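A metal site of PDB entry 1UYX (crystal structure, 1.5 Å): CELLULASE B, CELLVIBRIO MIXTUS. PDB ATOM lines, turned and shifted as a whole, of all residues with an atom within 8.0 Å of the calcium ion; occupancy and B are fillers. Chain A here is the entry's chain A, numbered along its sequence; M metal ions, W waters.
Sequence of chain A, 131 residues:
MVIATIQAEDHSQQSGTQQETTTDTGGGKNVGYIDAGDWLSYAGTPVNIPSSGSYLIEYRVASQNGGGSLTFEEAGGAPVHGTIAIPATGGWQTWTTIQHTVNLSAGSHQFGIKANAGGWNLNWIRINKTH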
ATOM      1  N   ILE A   6      30.974  15.261 -31.924  1.00  0.00           N
ATOM      2  CA  ILE A   6      30.402  16.577 -31.638  1.00  0.00           C
ATOM      3  C   ILE A   6      29.447  16.419 -30.472  1.00  0.00           C
ATOM      4  O   ILE A   6      28.457  15.703 -30.570  1.00  0.00           O
ATOM      5  CB  ILE A   6      29.651  17.110 -32.864  1.00  0.00           C
ATOM      6  CG1 ILE A   6      30.614  17.332 -34.041  1.00  0.00           C
ATOM      7  CG2 ILE A   6      28.913  18.413 -32.536  1.00  0.00           C
ATOM      8  CD1 ILE A   6      29.899  17.597 -35.356  1.00  0.00           C
ATOM      9  N   GLN A   7      29.741  17.065 -29.348  1.00  0.00           N
ATOM     10  CA  GLN A   7      28.773  17.114 -28.247  1.00  0.00           C
ATOM     11  C   GLN A   7      27.570  17.943 -28.692  1.00  0.00           C
ATOM     12  O   GLN A   7      27.712  19.014 -29.277  1.00  0.00           O
ATOM     13  CB  GLN A   7      29.424  17.712 -26.992  1.00  0.00           C
ATOM     14  CG  GLN A   7      30.530  16.840 -26.412  1.00  0.00           C
ATOM     15  CD  GLN A   7      30.020  15.483 -25.954  1.00  0.00           C
ATOM     16  OE1 GLN A   7      28.900  15.365 -25.452  1.00  0.00           O
ATOM     17  NE2 GLN A   7      30.834  14.447 -26.138  1.00  0.00           N
ATOM     18  N   ALA A   8      26.371  17.425 -28.453  1.00  0.00           N
ATOM     19  CA  ALA A   8      25.161  18.025 -29.006  1.00  0.00           C
ATOM     20  C   ALA A   8      24.929  19.454 -28.563  1.00  0.00           C
ATOM     21  O   ALA A   8      24.404  20.270 -29.325  1.00  0.00           O
ATOM     22  CB  ALA A   8      23.963  17.175 -28.657  1.00  0.00           C
ATOM     23  N   GLU A   9      25.323  19.741 -27.333  1.00  0.00           N
ATOM     24  CA  GLU A   9      25.210  21.069 -26.741  1.00  0.00           C
ATOM     25  C   GLU A   9      26.184  22.097 -27.304  1.00  0.00           C
ATOM     26  O   GLU A   9      26.002  23.288 -27.065  1.00  0.00           O
ATOM     27  CB  GLU A   9      25.371  20.966 -25.218  1.00  0.00           C
ATOM     28  CG  GLU A   9      26.782  20.677 -24.703  1.00  0.00           C
ATOM     29  CD  GLU A   9      27.123  19.208 -24.543  1.00  0.00           C
ATOM     30  OE1 GLU A   9      26.477  18.342 -25.179  1.00  0.00           O
ATOM     31  OE2 GLU A   9      28.072  18.907 -23.777  1.00  0.00           O
ATOM     32  N   ASP A  10      27.203  21.642 -28.045  1.00  0.00           N
ATOM     33  CA  ASP A  10      28.235  22.520 -28.609  1.00  0.00           C
ATOM     34  C   ASP A  10      27.845  23.074 -29.982  1.00  0.00           C
ATOM     35  O   ASP A  10      28.664  23.169 -30.899  1.00  0.00           O
ATOM     36  CB  ASP A  10      29.578  21.786 -28.716  1.00  0.00           C
ATOM     37  CG  ASP A  10      30.225  21.538 -27.371  1.00  0.00           C
ATOM     38  OD1 ASP A  10      29.735  22.036 -26.340  1.00  0.00           O
ATOM     39  OD2 ASP A  10      31.270  20.848 -27.279  1.00  0.00           O
ATOM     40  N   GLN A  19      19.666  23.062 -22.945  1.00  0.00           N
ATOM     41  CA  GLN A  19      20.673  22.196 -22.366  1.00  0.00           C
ATOM     42  C   GLN A  19      20.236  21.719 -20.982  1.00  0.00           C
ATOM     43  O   GLN A  19      19.513  22.426 -20.277  1.00  0.00           O
ATOM     44  CB  GLN A  19      21.940  23.028 -22.218  1.00  0.00           C
ATOM     45  CG  GLN A  19      23.142  22.332 -21.730  1.00  0.00           C
ATOM     46  CD  GLN A  19      24.324  23.279 -21.752  1.00  0.00           C
ATOM     47  OE1 GLN A  19      24.960  23.450 -22.791  1.00  0.00           O
ATOM     48  NE2 GLN A  19      24.569  23.937 -20.625  1.00  0.00           N
ATOM     49  N   GLU A  20      20.680  20.526 -20.603  1.00  0.00           N
ATOM     50  CA  GLU A  20      20.444  19.996 -19.258  1.00  0.00           C
ATOM     51  C   GLU A  20      21.535  19.000 -18.899  1.00  0.00           C
ATOM     52  O   GLU A  20      22.220  18.483 -19.759  1.00  0.00           O
ATOM     53  CB  GLU A  20      19.058  19.359 -19.150  1.00  0.00           C
ATOM     54  CG  GLU A  20      18.857  18.179 -20.091  1.00  0.00           C
ATOM     55  CD  GLU A  20      17.422  17.675 -20.150  1.00  0.00           C
ATOM     56  OE1 GLU A  20      16.525  18.245 -19.475  1.00  0.00           O
ATOM     57  OE2 GLU A  20      17.199  16.674 -20.875  1.00  0.00           O
ATOM     58  N   THR A  22      23.331  15.644 -17.988  1.00  0.00           N
ATOM     59  CA  THR A  22      23.134  14.230 -18.285  1.00  0.00           C
ATOM     60  C   THR A  22      23.869  13.337 -17.293  1.00  0.00           C
ATOM     61  O   THR A  22      24.972  13.688 -16.843  1.00  0.00           O
ATOM     62  CB  THR A  22      23.578  13.883 -19.736  1.00  0.00           C
ATOM     63  OG1 THR A  22      23.270  12.525 -20.023  1.00  0.00           O
ATOM     64  CG2 THR A  22      25.101  13.964 -19.932  1.00  0.00           C
ATOM     65  N   ASP A  24      24.495  10.187 -18.356  1.00  0.00           N
ATOM     66  CA  ASP A  24      25.186   9.260 -19.237  1.00  0.00           C
ATOM     67  C   ASP A  24      26.674   9.194 -18.900  1.00  0.00           C
ATOM     68  O   ASP A  24      27.213  10.084 -18.254  1.00  0.00           O
ATOM     69  CB  ASP A  24      25.007   9.721 -20.695  1.00  0.00           C
ATOM     70  CG  ASP A  24      25.327   8.642 -21.696  1.00  0.00           C
ATOM     71  OD1 ASP A  24      25.378   7.445 -21.335  1.00  0.00           O
ATOM     72  OD2 ASP A  24      25.544   8.913 -22.893  1.00  0.00           O
ATOM     73  N   THR A  25      27.327   8.114 -19.338  1.00  0.00           N
ATOM     74  CA  THR A  25      28.779   7.943 -19.214  1.00  0.00           C
ATOM     75  C   THR A  25      29.522   9.210 -19.656  1.00  0.00           C
ATOM     76  O   THR A  25      29.290   9.720 -20.762  1.00  0.00           O
ATOM     77  CB  THR A  25      29.229   6.752 -20.105  1.00  0.00           C
ATOM     78  OG1 THR A  25      28.414   5.599 -19.830  1.00  0.00           O
ATOM     79  CG2 THR A  25      30.647   6.290 -19.753  1.00  0.00           C
ATOM     80  N   GLY A  26      30.401   9.708 -18.797  1.00  0.00           N
ATOM     81  CA  GLY A  26      31.171  10.906 -19.075  1.00  0.00           C
ATOM     82  C   GLY A  26      30.549  12.204 -18.564  1.00  0.00           C
ATOM     83  O   GLY A  26      31.205  13.247 -18.562  1.00  0.00           O
ATOM     84  N   GLY A  27      29.287  12.135 -18.134  1.00  0.00           N
ATOM     85  CA  GLY A  27      28.582  13.294 -17.631  1.00  0.00           C
ATOM     86  C   GLY A  27      28.484  14.427 -18.648  1.00  0.00           C
ATOM     87  O   GLY A  27      28.400  14.187 -19.849  1.00  0.00           O
ATOM     88  N   GLY A  28      28.521  15.661 -18.160  1.00  0.00           N
ATOM     89  CA  GLY A  28      28.356  16.838 -18.984  1.00  0.00           C
ATOM     90  C   GLY A  28      26.891  17.171 -19.200  1.00  0.00           C
ATOM     91  O   GLY A  28      26.090  17.132 -18.265  1.00  0.00           O
ATOM     92  N   LYS A  29      26.553  17.507 -20.438  1.00  0.00           N
ATOM     93  CA  LYS A  29      25.215  17.992 -20.777  1.00  0.00           C
ATOM     94  C   LYS A  29      24.622  17.260 -21.976  1.00  0.00           C
ATOM     95  O   LYS A  29      25.346  16.736 -22.817  1.00  0.00           O
ATOM     96  CB  LYS A  29      25.264  19.482 -21.130  1.00  0.00           C
ATOM     97  CG  LYS A  29      25.886  20.385 -20.065  1.00  0.00           C
ATOM     98  CD  LYS A  29      24.996  20.503 -18.858  1.00  0.00           C
ATOM     99  CE  LYS A  29      25.526  21.526 -17.865  1.00  0.00           C
ATOM    100  NZ  LYS A  29      24.797  21.445 -16.573  1.00  0.00           N
ATOM    101  N   ASN A  30      23.294  17.233 -22.050  1.00  0.00           N
ATOM    102  CA  ASN A  30      22.593  16.835 -23.268  1.00  0.00           C
ATOM    103  C   ASN A  30      21.639  17.929 -23.709  1.00  0.00           C
ATOM    104  O   ASN A  30      21.322  18.827 -22.949  1.00  0.00           O
ATOM    105  CB  ASN A  30      21.875  15.479 -23.105  1.00  0.00           C
ATOM    106  CG  ASN A  30      20.669  15.550 -22.181  1.00  0.00           C
ATOM    107  OD1 ASN A  30      19.560  15.909 -22.603  1.00  0.00           O
ATOM    108  ND2 ASN A  30      20.859  15.178 -20.934  1.00  0.00           N
ATOM    109  N   VAL A  31      21.198  17.850 -24.966  1.00  0.00           N
ATOM    110  CA  VAL A  31      20.128  18.716 -25.459  1.00  0.00           C
ATOM    111  C   VAL A  31      18.811  18.052 -25.154  1.00  0.00           C
ATOM    112  O   VAL A  31      18.638  16.854 -25.374  1.00  0.00           O
ATOM    113  CB  VAL A  31      20.264  18.935 -26.973  1.00  0.00           C
ATOM    114  CG1 VAL A  31      19.089  19.775 -27.499  1.00  0.00           C
ATOM    115  CG2 VAL A  31      21.577  19.621 -27.280  1.00  0.00           C
ATOM    116  N   ARG A  60      23.879   9.512 -29.838  1.00  0.00           N
ATOM    117  CA  ARG A  60      23.689   9.045 -28.467  1.00  0.00           C
ATOM    118  C   ARG A  60      22.401   9.677 -27.970  1.00  0.00           C
ATOM    119  O   ARG A  60      22.340  10.892 -27.763  1.00  0.00           O
ATOM    120  CB  ARG A  60      24.891   9.455 -27.620  1.00  0.00           C
ATOM    121  CG  ARG A  60      24.900   8.873 -26.216  1.00  0.00           C
ATOM    122  CD  ARG A  60      25.052   7.365 -26.212  1.00  0.00           C
ATOM    123  NE  ARG A  60      25.239   6.849 -24.855  1.00  0.00           N
ATOM    124  CZ  ARG A  60      25.347   5.552 -24.556  1.00  0.00           C
ATOM    125  NH1 ARG A  60      25.273   4.628 -25.510  1.00  0.00           N
ATOM    126  NH2 ARG A  60      25.507   5.190 -23.297  1.00  0.00           N
ATOM    127  N   TRP A  95      20.345   5.728 -21.960  1.00  0.00           N
ATOM    128  CA  TRP A  95      21.028   6.086 -23.193  1.00  0.00           C
ATOM    129  C   TRP A  95      21.402   4.891 -24.053  1.00  0.00           C
ATOM    130  O   TRP A  95      21.761   3.817 -23.561  1.00  0.00           O
ATOM    131  CB  TRP A  95      22.273   6.907 -22.852  1.00  0.00           C
ATOM    132  CG  TRP A  95      21.925   8.200 -22.198  1.00  0.00           C
ATOM    133  CD1 TRP A  95      21.810   8.445 -20.860  1.00  0.00           C
ATOM    134  CD2 TRP A  95      21.560   9.406 -22.864  1.00  0.00           C
ATOM    135  NE1 TRP A  95      21.436   9.752 -20.660  1.00  0.00           N
ATOM    136  CE2 TRP A  95      21.259  10.364 -21.877  1.00  0.00           C
ATOM    137  CE3 TRP A  95      21.472   9.779 -24.212  1.00  0.00           C
ATOM    138  CZ2 TRP A  95      20.874  11.669 -22.185  1.00  0.00           C
ATOM    139  CZ3 TRP A  95      21.091  11.072 -24.515  1.00  0.00           C
ATOM    140  CH2 TRP A  95      20.793  12.004 -23.512  1.00  0.00           C
ATOM    141  N   LEU A 122      19.454  14.266 -26.809  1.00  0.00           N
ATOM    142  CA  LEU A 122      20.657  14.002 -27.600  1.00  0.00           C
ATOM    143  C   LEU A 122      21.917  14.434 -26.842  1.00  0.00           C
ATOM    144  O   LEU A 122      22.042  15.591 -26.470  1.00  0.00           O
ATOM    145  CB  LEU A 122      20.573  14.761 -28.917  1.00  0.00           C
ATOM    146  CG  LEU A 122      21.689  14.513 -29.935  1.00  0.00           C
ATOM    147  CD1 LEU A 122      21.699  13.082 -30.431  1.00  0.00           C
ATOM    148  CD2 LEU A 122      21.548  15.458 -31.122  1.00  0.00           C
ATOM    149  N   ASN A 123      22.840  13.487 -26.626  1.00  0.00           N
ATOM    150  CA  ASN A 123      24.075  13.763 -25.899  1.00  0.00           C
ATOM    151  C   ASN A 123      25.216  14.188 -26.833  1.00  0.00           C
ATOM    152  O   ASN A 123      25.882  15.191 -26.580  1.00  0.00           O
ATOM    153  CB  ASN A 123      24.464  12.523 -25.082  1.00  0.00           C
ATOM    154  CG  ASN A 123      25.571  12.782 -24.085  1.00  0.00           C
ATOM    155  OD1 ASN A 123      26.050  13.903 -23.951  1.00  0.00           O
ATOM    156  ND2 ASN A 123      25.994  11.727 -23.376  1.00  0.00           N
ATOM    157  N   TRP A 124      25.431  13.411 -27.890  1.00  0.00           N
ATOM    158  CA  TRP A 124      26.496  13.673 -28.860  1.00  0.00           C
ATOM    159  C   TRP A 124      26.221  12.952 -30.165  1.00  0.00           C
ATOM    160  O   TRP A 124      25.336  12.090 -30.247  1.00  0.00           O
ATOM    161  CB  TRP A 124      27.885  13.282 -28.309  1.00  0.00           C
ATOM    162  CG  TRP A 124      28.020  11.899 -27.671  1.00  0.00           C
ATOM    163  CD1 TRP A 124      28.085  11.625 -26.338  1.00  0.00           C
ATOM    164  CD2 TRP A 124      28.172  10.631 -28.337  1.00  0.00           C
ATOM    165  NE1 TRP A 124      28.236  10.278 -26.127  1.00  0.00           N
ATOM    166  CE2 TRP A 124      28.286   9.637 -27.339  1.00  0.00           C
ATOM    167  CE3 TRP A 124      28.193  10.227 -29.683  1.00  0.00           C
ATOM    168  CZ2 TRP A 124      28.425   8.277 -27.638  1.00  0.00           C
ATOM    169  CZ3 TRP A 124      28.326   8.880 -29.987  1.00  0.00           C
ATOM    170  CH2 TRP A 124      28.440   7.920 -28.964  1.00  0.00           C
ATOM    171  N   ILE A 125      26.976  13.321 -31.189  1.00  0.00           N
ATOM    172  CA  ILE A 125      26.936  12.753 -32.531  1.00  0.00           C
ATOM    173  C   ILE A 125      28.362  12.351 -32.875  1.00  0.00           C
ATOM    174  O   ILE A 125      29.322  13.021 -32.460  1.00  0.00           O
ATOM    175  CB  ILE A 125      26.429  13.797 -33.554  1.00  0.00           C
ATOM    176  CG1 ILE A 125      25.102  14.422 -33.095  1.00  0.00           C
ATOM    177  CG2 ILE A 125      26.320  13.202 -34.930  1.00  0.00           C
ATOM    178  CD1 ILE A 125      25.257  15.886 -32.673  1.00  0.00           C
HETATM  179 CA    CA M   1      26.831  15.924 -24.383  1.00  0.00          CA
HETATM  180  O   HOH W   1      28.440  16.156 -22.466  1.00  0.00           O
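Water W1 lies within hydrogen-bond range of the side-chain carboxylate (OE2) of Glu 9, the backbone NH (N) of Lys 29 and the backbone carbonyl oxygen (O) of Gly 27.
The calcium ion is bound by the side-chain amide oxygen of Asn 123, the backbone carbonyl oxygen of Lys 29, the side-chain amide oxygen of Gln 7, the backbone carbonyl oxygen of Asn 123, water W1 and the side-chain carboxylate of Glu 9. The calcium ion has six donor atoms within binding distance.
The backbone carbonyl oxygen (O) of Asn 123 lies close to the backbone NH (N) of Ala 8, at 3.0 Å. N of Asn 123 is in hydrogen-bond range of O of Arg 60, at 2.9 Å. OD2 of Asp 24 lies within hydrogen-bond range of ND2 of Asn 123, 2.9 Å away.
Within 4 Å of the calcium ion: Gln 7, Glu 9, Lys 29 and Asn 123.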
